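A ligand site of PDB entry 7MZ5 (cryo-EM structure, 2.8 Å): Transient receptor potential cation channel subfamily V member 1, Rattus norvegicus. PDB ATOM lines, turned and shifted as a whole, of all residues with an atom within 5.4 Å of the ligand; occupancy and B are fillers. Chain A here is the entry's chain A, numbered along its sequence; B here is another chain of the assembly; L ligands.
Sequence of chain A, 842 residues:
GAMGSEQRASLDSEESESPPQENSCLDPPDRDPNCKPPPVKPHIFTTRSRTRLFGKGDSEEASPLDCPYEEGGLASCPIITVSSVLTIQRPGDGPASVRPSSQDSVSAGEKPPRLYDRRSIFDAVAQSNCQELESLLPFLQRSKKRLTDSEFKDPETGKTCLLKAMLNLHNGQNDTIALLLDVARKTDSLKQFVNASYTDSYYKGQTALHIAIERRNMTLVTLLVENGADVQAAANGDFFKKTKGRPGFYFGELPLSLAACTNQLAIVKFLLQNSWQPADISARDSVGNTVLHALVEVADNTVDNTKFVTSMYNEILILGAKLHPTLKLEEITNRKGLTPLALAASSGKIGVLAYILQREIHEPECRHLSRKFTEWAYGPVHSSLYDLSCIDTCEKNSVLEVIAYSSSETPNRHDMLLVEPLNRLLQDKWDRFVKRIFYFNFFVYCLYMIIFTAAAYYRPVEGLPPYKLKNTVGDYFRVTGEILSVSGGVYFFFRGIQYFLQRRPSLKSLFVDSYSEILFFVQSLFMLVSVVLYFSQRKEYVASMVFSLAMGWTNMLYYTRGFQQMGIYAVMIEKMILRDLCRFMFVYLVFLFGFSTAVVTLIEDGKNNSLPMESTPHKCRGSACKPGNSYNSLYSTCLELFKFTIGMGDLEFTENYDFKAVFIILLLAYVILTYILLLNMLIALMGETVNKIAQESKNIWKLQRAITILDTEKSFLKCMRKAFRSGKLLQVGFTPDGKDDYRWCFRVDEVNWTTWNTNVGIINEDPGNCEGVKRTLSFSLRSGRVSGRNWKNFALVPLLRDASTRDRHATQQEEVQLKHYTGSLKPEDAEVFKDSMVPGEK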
ATOM      1  N   PHE A 511      18.071  24.059  23.350  1.00  0.00           N
ATOM      2  CA  PHE A 511      16.720  24.594  23.464  1.00  0.00           C
ATOM      3  C   PHE A 511      16.109  24.997  22.130  1.00  0.00           C
ATOM      4  O   PHE A 511      14.884  25.048  22.023  1.00  0.00           O
ATOM      5  CB  PHE A 511      16.725  25.821  24.382  1.00  0.00           C
ATOM      6  CG  PHE A 511      16.964  25.492  25.824  1.00  0.00           C
ATOM      7  CD1 PHE A 511      18.261  25.433  26.323  1.00  0.00           C
ATOM      8  CD2 PHE A 511      15.910  25.234  26.675  1.00  0.00           C
ATOM      9  CE1 PHE A 511      18.486  25.131  27.655  1.00  0.00           C
ATOM     10  CE2 PHE A 511      16.135  24.932  28.007  1.00  0.00           C
ATOM     11  CZ  PHE A 511      17.425  24.880  28.492  1.00  0.00           C
ATOM     12  N   TYR A 515      12.800  21.418  22.312  1.00  0.00           N
ATOM     13  CA  TYR A 515      12.181  22.259  23.332  1.00  0.00           C
ATOM     14  C   TYR A 515      11.076  21.504  24.063  1.00  0.00           C
ATOM     15  O   TYR A 515      11.028  21.501  25.299  1.00  0.00           O
ATOM     16  CB  TYR A 515      11.613  23.514  22.678  1.00  0.00           C
ATOM     17  CG  TYR A 515      10.850  24.419  23.616  1.00  0.00           C
ATOM     18  CD1 TYR A 515      11.519  25.263  24.506  1.00  0.00           C
ATOM     19  CD2 TYR A 515       9.471  24.450  23.608  1.00  0.00           C
ATOM     20  CE1 TYR A 515      10.827  26.086  25.356  1.00  0.00           C
ATOM     21  CE2 TYR A 515       8.769  25.282  24.455  1.00  0.00           C
ATOM     22  CZ  TYR A 515       9.448  26.095  25.329  1.00  0.00           C
ATOM     23  OH  TYR A 515       8.747  26.917  26.177  1.00  0.00           O
ATOM     24  N   SER A 516      10.197  20.841  23.315  1.00  0.00           N
ATOM     25  CA  SER A 516       9.112  20.088  23.947  1.00  0.00           C
ATOM     26  C   SER A 516       9.670  18.920  24.759  1.00  0.00           C
ATOM     27  O   SER A 516       9.163  18.628  25.849  1.00  0.00           O
ATOM     28  CB  SER A 516       8.146  19.580  22.877  1.00  0.00           C
ATOM     29  OG  SER A 516       8.822  18.803  21.914  1.00  0.00           O
ATOM     30  N   ILE A 518      12.581  18.866  26.241  1.00  0.00           N
ATOM     31  CA  ILE A 518      13.155  19.428  27.457  1.00  0.00           C
ATOM     32  C   ILE A 518      12.056  19.758  28.453  1.00  0.00           C
ATOM     33  O   ILE A 518      12.217  19.556  29.663  1.00  0.00           O
ATOM     34  CB  ILE A 518      14.007  20.670  27.117  1.00  0.00           C
ATOM     35  CG1 ILE A 518      15.325  20.209  26.514  1.00  0.00           C
ATOM     36  CG2 ILE A 518      14.269  21.511  28.373  1.00  0.00           C
ATOM     37  CD1 ILE A 518      16.020  21.258  25.717  1.00  0.00           C
ATOM     38  N   LEU A 519      10.934  20.320  27.976  1.00  0.00           N
ATOM     39  CA  LEU A 519       9.856  20.645  28.906  1.00  0.00           C
ATOM     40  C   LEU A 519       9.266  19.389  29.540  1.00  0.00           C
ATOM     41  O   LEU A 519       8.995  19.373  30.748  1.00  0.00           O
ATOM     42  CB  LEU A 519       8.763  21.427  28.182  1.00  0.00           C
ATOM     43  CG  LEU A 519       9.078  22.863  27.764  1.00  0.00           C
ATOM     44  CD1 LEU A 519       7.862  23.439  27.067  1.00  0.00           C
ATOM     45  CD2 LEU A 519       9.475  23.724  28.945  1.00  0.00           C
ATOM     46  N   PHE A 520       9.078  18.325  28.753  1.00  0.00           N
ATOM     47  CA  PHE A 520       8.579  17.084  29.321  1.00  0.00           C
ATOM     48  C   PHE A 520       9.573  16.512  30.325  1.00  0.00           C
ATOM     49  O   PHE A 520       9.177  16.029  31.399  1.00  0.00           O
ATOM     50  CB  PHE A 520       8.297  16.065  28.228  1.00  0.00           C
ATOM     51  CG  PHE A 520       6.940  16.195  27.611  1.00  0.00           C
ATOM     52  CD1 PHE A 520       5.812  15.755  28.283  1.00  0.00           C
ATOM     53  CD2 PHE A 520       6.783  16.727  26.349  1.00  0.00           C
ATOM     54  CE1 PHE A 520       4.569  15.875  27.713  1.00  0.00           C
ATOM     55  CE2 PHE A 520       5.540  16.846  25.779  1.00  0.00           C
ATOM     56  CZ  PHE A 520       4.431  16.410  26.456  1.00  0.00           C
ATOM     57  N   VAL A 522      11.838  18.160  32.108  1.00  0.00           N
ATOM     58  CA  VAL A 522      11.886  18.987  33.307  1.00  0.00           C
ATOM     59  C   VAL A 522      10.626  18.772  34.153  1.00  0.00           C
ATOM     60  O   VAL A 522      10.680  18.792  35.388  1.00  0.00           O
ATOM     61  CB  VAL A 522      12.072  20.473  32.940  1.00  0.00           C
ATOM     62  CG1 VAL A 522      11.942  21.351  34.174  1.00  0.00           C
ATOM     63  CG2 VAL A 522      13.435  20.694  32.305  1.00  0.00           C
ATOM     64  N   PHE A 547       4.676  22.690  40.404  1.00  0.00           N
ATOM     65  CA  PHE A 547       5.361  23.103  39.184  1.00  0.00           C
ATOM     66  C   PHE A 547       5.216  22.045  38.116  1.00  0.00           C
ATOM     67  O   PHE A 547       4.789  22.343  36.994  1.00  0.00           O
ATOM     68  CB  PHE A 547       6.845  23.377  39.446  1.00  0.00           C
ATOM     69  CG  PHE A 547       7.132  24.742  39.991  1.00  0.00           C
ATOM     70  CD1 PHE A 547       6.801  25.880  39.284  1.00  0.00           C
ATOM     71  CD2 PHE A 547       7.770  24.899  41.212  1.00  0.00           C
ATOM     72  CE1 PHE A 547       7.058  27.134  39.775  1.00  0.00           C
ATOM     73  CE2 PHE A 547       8.035  26.155  41.716  1.00  0.00           C
ATOM     74  CZ  PHE A 547       7.681  27.267  40.992  1.00  0.00           C
ATOM     75  N   ALA A 550       1.747  22.282  36.835  1.00  0.00           N
ATOM     76  CA  ALA A 550       1.615  23.391  35.909  1.00  0.00           C
ATOM     77  C   ALA A 550       2.273  23.050  34.595  1.00  0.00           C
ATOM     78  O   ALA A 550       1.633  23.114  33.537  1.00  0.00           O
ATOM     79  CB  ALA A 550       2.231  24.652  36.502  1.00  0.00           C
ATOM     80  N   MET A 551       3.504  22.519  34.663  1.00  0.00           N
ATOM     81  CA  MET A 551       4.216  22.195  33.439  1.00  0.00           C
ATOM     82  C   MET A 551       3.452  21.147  32.658  1.00  0.00           C
ATOM     83  O   MET A 551       3.273  21.285  31.436  1.00  0.00           O
ATOM     84  CB  MET A 551       5.618  21.703  33.758  1.00  0.00           C
ATOM     85  CG  MET A 551       6.531  22.802  34.267  1.00  0.00           C
ATOM     86  SD  MET A 551       8.243  22.307  34.369  1.00  0.00           S
ATOM     87  CE  MET A 551       8.651  22.212  32.633  1.00  0.00           C
ATOM     88  N   THR A 554       0.704  22.735  30.715  1.00  0.00           N
ATOM     89  CA  THR A 554       1.230  23.493  29.590  1.00  0.00           C
ATOM     90  C   THR A 554       1.872  22.574  28.572  1.00  0.00           C
ATOM     91  O   THR A 554       1.868  22.889  27.373  1.00  0.00           O
ATOM     92  CB  THR A 554       2.219  24.539  30.084  1.00  0.00           C
ATOM     93  OG1 THR A 554       3.273  23.915  30.817  1.00  0.00           O
ATOM     94  CG2 THR A 554       1.517  25.558  30.970  1.00  0.00           C
ATOM     95  N   ASN A 555       2.331  21.391  28.987  1.00  0.00           N
ATOM     96  CA  ASN A 555       2.913  20.480  28.024  1.00  0.00           C
ATOM     97  C   ASN A 555       1.865  19.895  27.091  1.00  0.00           C
ATOM     98  O   ASN A 555       2.233  19.295  26.070  1.00  0.00           O
ATOM     99  CB  ASN A 555       3.668  19.369  28.748  1.00  0.00           C
ATOM    100  CG  ASN A 555       4.980  19.838  29.331  1.00  0.00           C
ATOM    101  OD1 ASN A 555       5.516  20.869  28.926  1.00  0.00           O
ATOM    102  ND2 ASN A 555       5.513  19.088  30.275  1.00  0.00           N
ATOM    103  N   LEU A 557       0.345  21.652  25.125  1.00  0.00           N
ATOM    104  CA  LEU A 557       0.599  22.361  23.875  1.00  0.00           C
ATOM    105  C   LEU A 557       1.467  21.559  22.921  1.00  0.00           C
ATOM    106  O   LEU A 557       1.370  21.760  21.711  1.00  0.00           O
ATOM    107  CB  LEU A 557       1.257  23.705  24.150  1.00  0.00           C
ATOM    108  CG  LEU A 557       0.276  24.872  24.308  1.00  0.00           C
ATOM    109  CD1 LEU A 557      -0.588  24.690  25.539  1.00  0.00           C
ATOM    110  CD2 LEU A 557       1.028  26.183  24.362  1.00  0.00           C
ATOM    111  N   TYR A 558       2.288  20.637  23.433  1.00  0.00           N
ATOM    112  CA  TYR A 558       3.042  19.767  22.542  1.00  0.00           C
ATOM    113  C   TYR A 558       2.115  18.988  21.629  1.00  0.00           C
ATOM    114  O   TYR A 558       2.389  18.832  20.434  1.00  0.00           O
ATOM    115  CB  TYR A 558       3.918  18.803  23.347  1.00  0.00           C
ATOM    116  CG  TYR A 558       4.431  17.655  22.526  1.00  0.00           C
ATOM    117  CD1 TYR A 558       5.472  17.825  21.624  1.00  0.00           C
ATOM    118  CD2 TYR A 558       3.873  16.387  22.645  1.00  0.00           C
ATOM    119  CE1 TYR A 558       5.938  16.770  20.876  1.00  0.00           C
ATOM    120  CE2 TYR A 558       4.328  15.340  21.892  1.00  0.00           C
ATOM    121  CZ  TYR A 558       5.360  15.531  21.008  1.00  0.00           C
ATOM    122  OH  TYR A 558       5.826  14.476  20.260  1.00  0.00           O
ATOM    123  N   ARG A 561       0.691  21.113  18.733  1.00  0.00           N
ATOM    124  CA  ARG A 561       1.535  21.145  17.548  1.00  0.00           C
ATOM    125  C   ARG A 561       1.306  19.888  16.719  1.00  0.00           C
ATOM    126  O   ARG A 561       1.240  18.782  17.257  1.00  0.00           O
ATOM    127  CB  ARG A 561       3.003  21.250  17.953  1.00  0.00           C
ATOM    128  CG  ARG A 561       3.344  22.454  18.820  1.00  0.00           C
ATOM    129  CD  ARG A 561       4.785  22.391  19.301  1.00  0.00           C
ATOM    130  NE  ARG A 561       5.723  22.372  18.180  1.00  0.00           N
ATOM    131  CZ  ARG A 561       7.046  22.378  18.315  1.00  0.00           C
ATOM    132  NH1 ARG A 561       7.629  22.440  19.493  1.00  0.00           N
ATOM    133  NH2 ARG A 561       7.801  22.327  17.222  1.00  0.00           N
ATOM    134  N   ALA A 570       1.175  27.295  19.678  1.00  0.00           N
ATOM    135  CA  ALA A 570       2.216  26.723  20.529  1.00  0.00           C
ATOM    136  C   ALA A 570       3.593  26.971  19.939  1.00  0.00           C
ATOM    137  O   ALA A 570       4.552  27.238  20.676  1.00  0.00           O
ATOM    138  CB  ALA A 570       1.976  25.219  20.702  1.00  0.00           C
ATOM    139  N   VAL A 571       3.711  26.913  18.614  1.00  0.00           N
ATOM    140  CA  VAL A 571       4.990  27.223  17.967  1.00  0.00           C
ATOM    141  C   VAL A 571       5.405  28.649  18.265  1.00  0.00           C
ATOM    142  O   VAL A 571       6.580  28.928  18.566  1.00  0.00           O
ATOM    143  CB  VAL A 571       4.892  26.964  16.451  1.00  0.00           C
ATOM    144  CG1 VAL A 571       6.058  27.615  15.714  1.00  0.00           C
ATOM    145  CG2 VAL A 571       4.836  25.477  16.187  1.00  0.00           C
ATOM    146  N   ILE A 573       4.521  30.493  20.793  1.00  0.00           N
ATOM    147  CA  ILE A 573       4.908  30.606  22.201  1.00  0.00           C
ATOM    148  C   ILE A 573       6.337  30.124  22.391  1.00  0.00           C
ATOM    149  O   ILE A 573       7.144  30.772  23.076  1.00  0.00           O
ATOM    150  CB  ILE A 573       3.940  29.816  23.094  1.00  0.00           C
ATOM    151  CG1 ILE A 573       2.547  30.431  23.063  1.00  0.00           C
ATOM    152  CG2 ILE A 573       4.457  29.797  24.530  1.00  0.00           C
ATOM    153  CD1 ILE A 573       1.474  29.487  23.513  1.00  0.00           C
ATOM    154  N   GLU A 574       6.670  28.969  21.818  1.00  0.00           N
ATOM    155  CA  GLU A 574       8.017  28.437  21.923  1.00  0.00           C
ATOM    156  C   GLU A 574       9.044  29.414  21.362  1.00  0.00           C
ATOM    157  O   GLU A 574      10.074  29.699  21.994  1.00  0.00           O
ATOM    158  CB  GLU A 574       8.097  27.092  21.209  1.00  0.00           C
ATOM    159  CG  GLU A 574       9.507  26.557  20.934  1.00  0.00           C
ATOM    160  CD  GLU A 574       9.491  25.162  20.351  1.00  0.00           C
ATOM    161  OE1 GLU A 574       8.397  24.570  20.233  1.00  0.00           O
ATOM    162  OE2 GLU A 574      10.571  24.647  20.002  1.00  0.00           O
ATOM    163  N   ILE A 577       9.426  32.557  23.583  1.00  0.00           N
ATOM    164  CA  ILE A 577      10.150  32.280  24.829  1.00  0.00           C
ATOM    165  C   ILE A 577      11.637  32.111  24.554  1.00  0.00           C
ATOM    166  O   ILE A 577      12.470  32.664  25.274  1.00  0.00           O
ATOM    167  CB  ILE A 577       9.544  31.060  25.529  1.00  0.00           C
ATOM    168  CG1 ILE A 577       8.169  31.408  26.100  1.00  0.00           C
ATOM    169  CG2 ILE A 577      10.479  30.574  26.646  1.00  0.00           C
ATOM    170  CD1 ILE A 577       7.331  30.213  26.473  1.00  0.00           C
ATOM    171  N   LEU A 578      11.991  31.365  23.518  1.00  0.00           N
ATOM    172  CA  LEU A 578      13.401  31.087  23.279  1.00  0.00           C
ATOM    173  C   LEU A 578      14.134  32.286  22.694  1.00  0.00           C
ATOM    174  O   LEU A 578      15.273  32.569  23.077  1.00  0.00           O
ATOM    175  CB  LEU A 578      13.555  29.890  22.347  1.00  0.00           C
ATOM    176  CG  LEU A 578      13.030  28.550  22.881  1.00  0.00           C
ATOM    177  CD1 LEU A 578      13.142  27.494  21.800  1.00  0.00           C
ATOM    178  CD2 LEU A 578      13.778  28.135  24.123  1.00  0.00           C
ATOM    179  N   LEU A 581      12.037  36.517  24.477  1.00  0.00           N
ATOM    180  CA  LEU A 581      11.783  36.780  25.893  1.00  0.00           C
ATOM    181  C   LEU A 581      13.040  37.257  26.616  1.00  0.00           C
ATOM    182  O   LEU A 581      12.931  38.036  27.559  1.00  0.00           O
ATOM    183  CB  LEU A 581      11.233  35.524  26.571  1.00  0.00           C
ATOM    184  CG  LEU A 581      10.767  35.662  28.022  1.00  0.00           C
ATOM    185  CD1 LEU A 581       9.603  36.626  28.125  1.00  0.00           C
ATOM    186  CD2 LEU A 581      10.384  34.313  28.581  1.00  0.00           C
ATOM    187  N   PHE B 591      -3.337  27.082  29.857  1.00  0.00           N
ATOM    188  CA  PHE B 591      -2.459  27.777  30.803  1.00  0.00           C
ATOM    189  C   PHE B 591      -3.206  28.153  32.076  1.00  0.00           C
ATOM    190  O   PHE B 591      -2.685  27.956  33.179  1.00  0.00           O
ATOM    191  CB  PHE B 591      -1.876  29.031  30.156  1.00  0.00           C
ATOM    192  CG  PHE B 591      -0.649  28.768  29.332  1.00  0.00           C
ATOM    193  CD1 PHE B 591      -0.749  28.184  28.100  1.00  0.00           C
ATOM    194  CD2 PHE B 591       0.597  29.125  29.808  1.00  0.00           C
ATOM    195  CE1 PHE B 591       0.368  27.944  27.345  1.00  0.00           C
ATOM    196  CE2 PHE B 591       1.726  28.886  29.046  1.00  0.00           C
ATOM    197  CZ  PHE B 591       1.605  28.300  27.818  1.00  0.00           C
ATOM    198  N   PHE B 595      -2.161  26.525  35.701  1.00  0.00           N
ATOM    199  CA  PHE B 595      -1.642  27.340  36.787  1.00  0.00           C
ATOM    200  C   PHE B 595      -2.647  27.484  37.921  1.00  0.00           C
ATOM    201  O   PHE B 595      -2.242  27.582  39.072  1.00  0.00           O
ATOM    202  CB  PHE B 595      -1.206  28.699  36.255  1.00  0.00           C
ATOM    203  CG  PHE B 595       0.162  28.669  35.639  1.00  0.00           C
ATOM    204  CD1 PHE B 595       1.290  28.791  36.419  1.00  0.00           C
ATOM    205  CD2 PHE B 595       0.312  28.499  34.269  1.00  0.00           C
ATOM    206  CE1 PHE B 595       2.537  28.751  35.859  1.00  0.00           C
ATOM    207  CE2 PHE B 595       1.567  28.461  33.712  1.00  0.00           C
ATOM    208  CZ  PHE B 595       2.682  28.591  34.497  1.00  0.00           C
ATOM    209  N   LEU B 666       4.785  31.036  40.715  1.00  0.00           N
ATOM    210  CA  LEU B 666       3.724  30.520  39.857  1.00  0.00           C
ATOM    211  C   LEU B 666       2.890  31.655  39.275  1.00  0.00           C
ATOM    212  O   LEU B 666       2.588  31.657  38.076  1.00  0.00           O
ATOM    213  CB  LEU B 666       2.819  29.562  40.634  1.00  0.00           C
ATOM    214  CG  LEU B 666       3.317  28.143  40.877  1.00  0.00           C
ATOM    215  CD1 LEU B 666       2.372  27.432  41.824  1.00  0.00           C
ATOM    216  CD2 LEU B 666       3.438  27.368  39.580  1.00  0.00           C
ATOM    217  N   LEU B 668       3.726  34.846  38.872  1.00  0.00           N
ATOM    218  CA  LEU B 668       4.517  35.638  37.934  1.00  0.00           C
ATOM    219  C   LEU B 668       4.712  34.901  36.616  1.00  0.00           C
ATOM    220  O   LEU B 668       4.653  35.508  35.547  1.00  0.00           O
ATOM    221  CB  LEU B 668       5.866  35.995  38.557  1.00  0.00           C
ATOM    222  CG  LEU B 668       5.845  36.982  39.724  1.00  0.00           C
ATOM    223  CD1 LEU B 668       7.212  37.059  40.372  1.00  0.00           C
ATOM    224  CD2 LEU B 668       5.401  38.354  39.260  1.00  0.00           C
ATOM    225  N   ALA B 669       4.962  33.592  36.678  1.00  0.00           N
ATOM    226  CA  ALA B 669       5.082  32.815  35.455  1.00  0.00           C
ATOM    227  C   ALA B 669       3.771  32.822  34.682  1.00  0.00           C
ATOM    228  O   ALA B 669       3.768  32.931  33.455  1.00  0.00           O
ATOM    229  CB  ALA B 669       5.504  31.384  35.780  1.00  0.00           C
ATOM    230  N   ILE B 672       3.445  36.332  33.028  1.00  0.00           N
ATOM    231  CA  ILE B 672       4.346  36.499  31.894  1.00  0.00           C
ATOM    232  C   ILE B 672       3.889  35.633  30.736  1.00  0.00           C
ATOM    233  O   ILE B 672       3.873  36.083  29.576  1.00  0.00           O
ATOM    234  CB  ILE B 672       5.796  36.177  32.311  1.00  0.00           C
ATOM    235  CG1 ILE B 672       6.298  37.207  33.336  1.00  0.00           C
ATOM    236  CG2 ILE B 672       6.705  36.184  31.095  1.00  0.00           C
ATOM    237  CD1 ILE B 672       7.457  36.729  34.166  1.00  0.00           C
ATOM    238  N   LEU B 673       3.501  34.395  31.012  1.00  0.00           N
ATOM    239  CA  LEU B 673       3.047  33.501  29.962  1.00  0.00           C
ATOM    240  C   LEU B 673       1.746  33.994  29.348  1.00  0.00           C
ATOM    241  O   LEU B 673       1.569  33.919  28.131  1.00  0.00           O
ATOM    242  CB  LEU B 673       2.880  32.088  30.509  1.00  0.00           C
ATOM    243  CG  LEU B 673       4.206  31.398  30.870  1.00  0.00           C
ATOM    244  CD1 LEU B 673       3.957  30.206  31.775  1.00  0.00           C
ATOM    245  CD2 LEU B 673       4.962  30.986  29.623  1.00  0.00           C
ATOM    246  N   ILE B 676       2.525  36.795  27.125  1.00  0.00           N
ATOM    247  CA  ILE B 676       3.097  36.201  25.917  1.00  0.00           C
ATOM    248  C   ILE B 676       1.988  35.654  25.025  1.00  0.00           C
ATOM    249  O   ILE B 676       2.047  35.781  23.794  1.00  0.00           O
ATOM    250  CB  ILE B 676       4.122  35.109  26.304  1.00  0.00           C
ATOM    251  CG1 ILE B 676       5.402  35.760  26.823  1.00  0.00           C
ATOM    252  CG2 ILE B 676       4.421  34.188  25.126  1.00  0.00           C
ATOM    253  CD1 ILE B 676       6.291  34.839  27.629  1.00  0.00           C
HETATM  254  C1  LIG L   1       5.788  20.805  25.780  1.00  0.00           C
HETATM  255  O1  LIG L   1       6.151  21.417  24.539  1.00  0.00           O
HETATM  256  C2  LIG L   1       5.655  22.659  24.246  1.00  0.00           C
HETATM  257  C3  LIG L   1       5.076  23.432  25.240  1.00  0.00           C
HETATM  258  C4  LIG L   1       5.757  23.150  22.952  1.00  0.00           C
HETATM  259  O2  LIG L   1       6.335  22.391  21.988  1.00  0.00           O
HETATM  260  C5  LIG L   1       5.271  24.413  22.650  1.00  0.00           C
HETATM  261  C6  LIG L   1       4.696  25.185  23.635  1.00  0.00           C
HETATM  262  C7  LIG L   1       4.593  24.694  24.929  1.00  0.00           C
HETATM  263  C8  LIG L   1       3.955  25.549  26.004  1.00  0.00           C
HETATM  264  C9  LIG L   1       4.936  25.868  27.091  1.00  0.00           C
HETATM  265  O3  LIG L   1       5.324  24.997  27.851  1.00  0.00           O
HETATM  266  O4  LIG L   1       5.439  27.228  27.243  1.00  0.00           O
HETATM  267  C10 LIG L   1       5.284  27.932  28.481  1.00  0.00           C
HETATM  268  C11 LIG L   1       6.158  27.276  29.506  1.00  0.00           C
HETATM  269  C12 LIG L   1       7.486  27.435  29.369  1.00  0.00           C
HETATM  270  C13 LIG L   1       8.586  26.852  30.240  1.00  0.00           C
HETATM  271  C14 LIG L   1       5.425  26.483  30.568  1.00  0.00           C
HETATM  272  C15 LIG L   1       6.248  26.250  31.811  1.00  0.00           C
HETATM  273  O5  LIG L   1       6.947  24.999  31.685  1.00  0.00           O
HETATM  274  C16 LIG L   1       5.381  26.158  33.035  1.00  0.00           C
HETATM  275  O6  LIG L   1       4.355  25.495  33.113  1.00  0.00           O
HETATM  276  C17 LIG L   1       5.943  26.956  34.094  1.00  0.00           C
HETATM  277  C18 LIG L   1       5.445  26.965  35.513  1.00  0.00           C
HETATM  278  C19 LIG L   1       6.968  27.671  33.645  1.00  0.00           C
HETATM  279  C20 LIG L   1       7.129  27.459  32.155  1.00  0.00           C
HETATM  280  C21 LIG L   1       8.566  27.322  31.683  1.00  0.00           C
HETATM  281  O7  LIG L   1       9.161  28.617  31.774  1.00  0.00           O
HETATM  282  C22 LIG L   1       9.409  26.345  32.500  1.00  0.00           C
HETATM  283  C23 LIG L   1      10.064  26.970  33.726  1.00  0.00           C
HETATM  284  C24 LIG L   1      10.500  25.732  31.614  1.00  0.00           C
HETATM  285  C25 LIG L   1      11.006  26.764  30.612  1.00  0.00           C
HETATM  286  C26 LIG L   1      12.225  26.255  29.876  1.00  0.00           C
HETATM  287  C27 LIG L   1      12.695  25.056  30.126  1.00  0.00           C
HETATM  288  C28 LIG L   1      12.894  27.137  28.872  1.00  0.00           C
HETATM  289  O8  LIG L   1      11.325  27.974  31.272  1.00  0.00           O
HETATM  290  C29 LIG L   1       9.932  27.196  29.633  1.00  0.00           C
HETATM  291  O9  LIG L   1       9.991  28.625  29.640  1.00  0.00           O
HETATM  292  C30 LIG L   1      10.312  28.926  30.992  1.00  0.00           C
HETATM  293  C31 LIG L   1      10.774  30.365  31.167  1.00  0.00           C
HETATM  294  C32 LIG L   1       9.581  31.247  31.477  1.00  0.00           C
HETATM  295  C33 LIG L   1       8.865  31.842  30.453  1.00  0.00           C
HETATM  296  C34 LIG L   1       7.775  32.645  30.748  1.00  0.00           C
HETATM  297  C35 LIG L   1       7.399  32.871  32.064  1.00  0.00           C
HETATM  298  C36 LIG L   1       8.116  32.275  33.088  1.00  0.00           C
HETATM  299  C37 LIG L   1       9.207  31.463  32.794  1.00  0.00           C
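Ser 516 touches the ligand.
CD1 of Leu 519 touches O3 of the ligand, 3.1 Å away.
CE2 of Phe 520 touches C1 of the ligand (3.97 Å).
Ala 550 touches the ligand.
OD1 of Asn 555 touches C1 of the ligand, at 3.2 Å.
Leu 557 touches the ligand (CD2 to C8, 3.4 Å).
CB of Tyr 558 touches O1 of the ligand, 3.6 Å away.
Ala 570 touches the ligand (O to C5, 3.5 Å).
CG2 of Ile 573 touches O4 of the ligand, at 3.9 Å.
CG2 of Ile 577 touches O9 of the ligand, 3.6 Å away.
Leu 581 touches the ligand.
CE2 of Phe 591 of chain B touches C10 of the ligand, 3.7 Å away.
Phe 595 of chain B touches the ligand.
Ala 669 of chain B touches the ligand (CB to C36, 3.9 Å).
CG2 of Ile 672 of chain B touches C35 of the ligand (3.5 Å).
Leu 673 of chain B touches the ligand (CD2 to C10, 3.3 Å).
Hydrophobic or aromatic side chains that line the ligand: Tyr 515, Leu 519, Phe 520, Met 551, Leu 557, Tyr 558, Ala 570, Ile 573, Ile 577, Leu 581, Phe 591 of chain B, Phe 595 of chain B, Ala 669 of chain B, Ile 672 of chain B and Leu 673 of chain B.
OG1 of Thr 554 lies within hydrogen-bond range of O6 of the ligand.
NH1 of Arg 561 lies within hydrogen-bond range of O2 of the ligand, 2.8 Å away.
OH of Tyr 515 lies close to O4 of the ligand (3.5 Å).
N of Met 551 lies close to O6 of the ligand.
The side-chain carboxylate (OE1) of Glu 574 lies within hydrogen-bond range of an oxygen (O2) of the ligand (3.5 Å).
O of Ala 550 lies within hydrogen-bond range of OG1 of Thr 554, at 3.3 Å.
The side-chain hydroxyl of Thr 554 is in hydrogen-bond range of the backbone carbonyl oxygen of Met 551 (2.7 Å).
The guanidinium group (NH1) of Arg 561 lies within salt-bridge range of the side-chain carboxylate (OE2) of Glu 574 (3.7 Å).
The side-chain amide nitrogen (ND2) of Asn 555 sits close to the backbone carbonyl oxygen (O) of Met 551 (3.3 Å).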
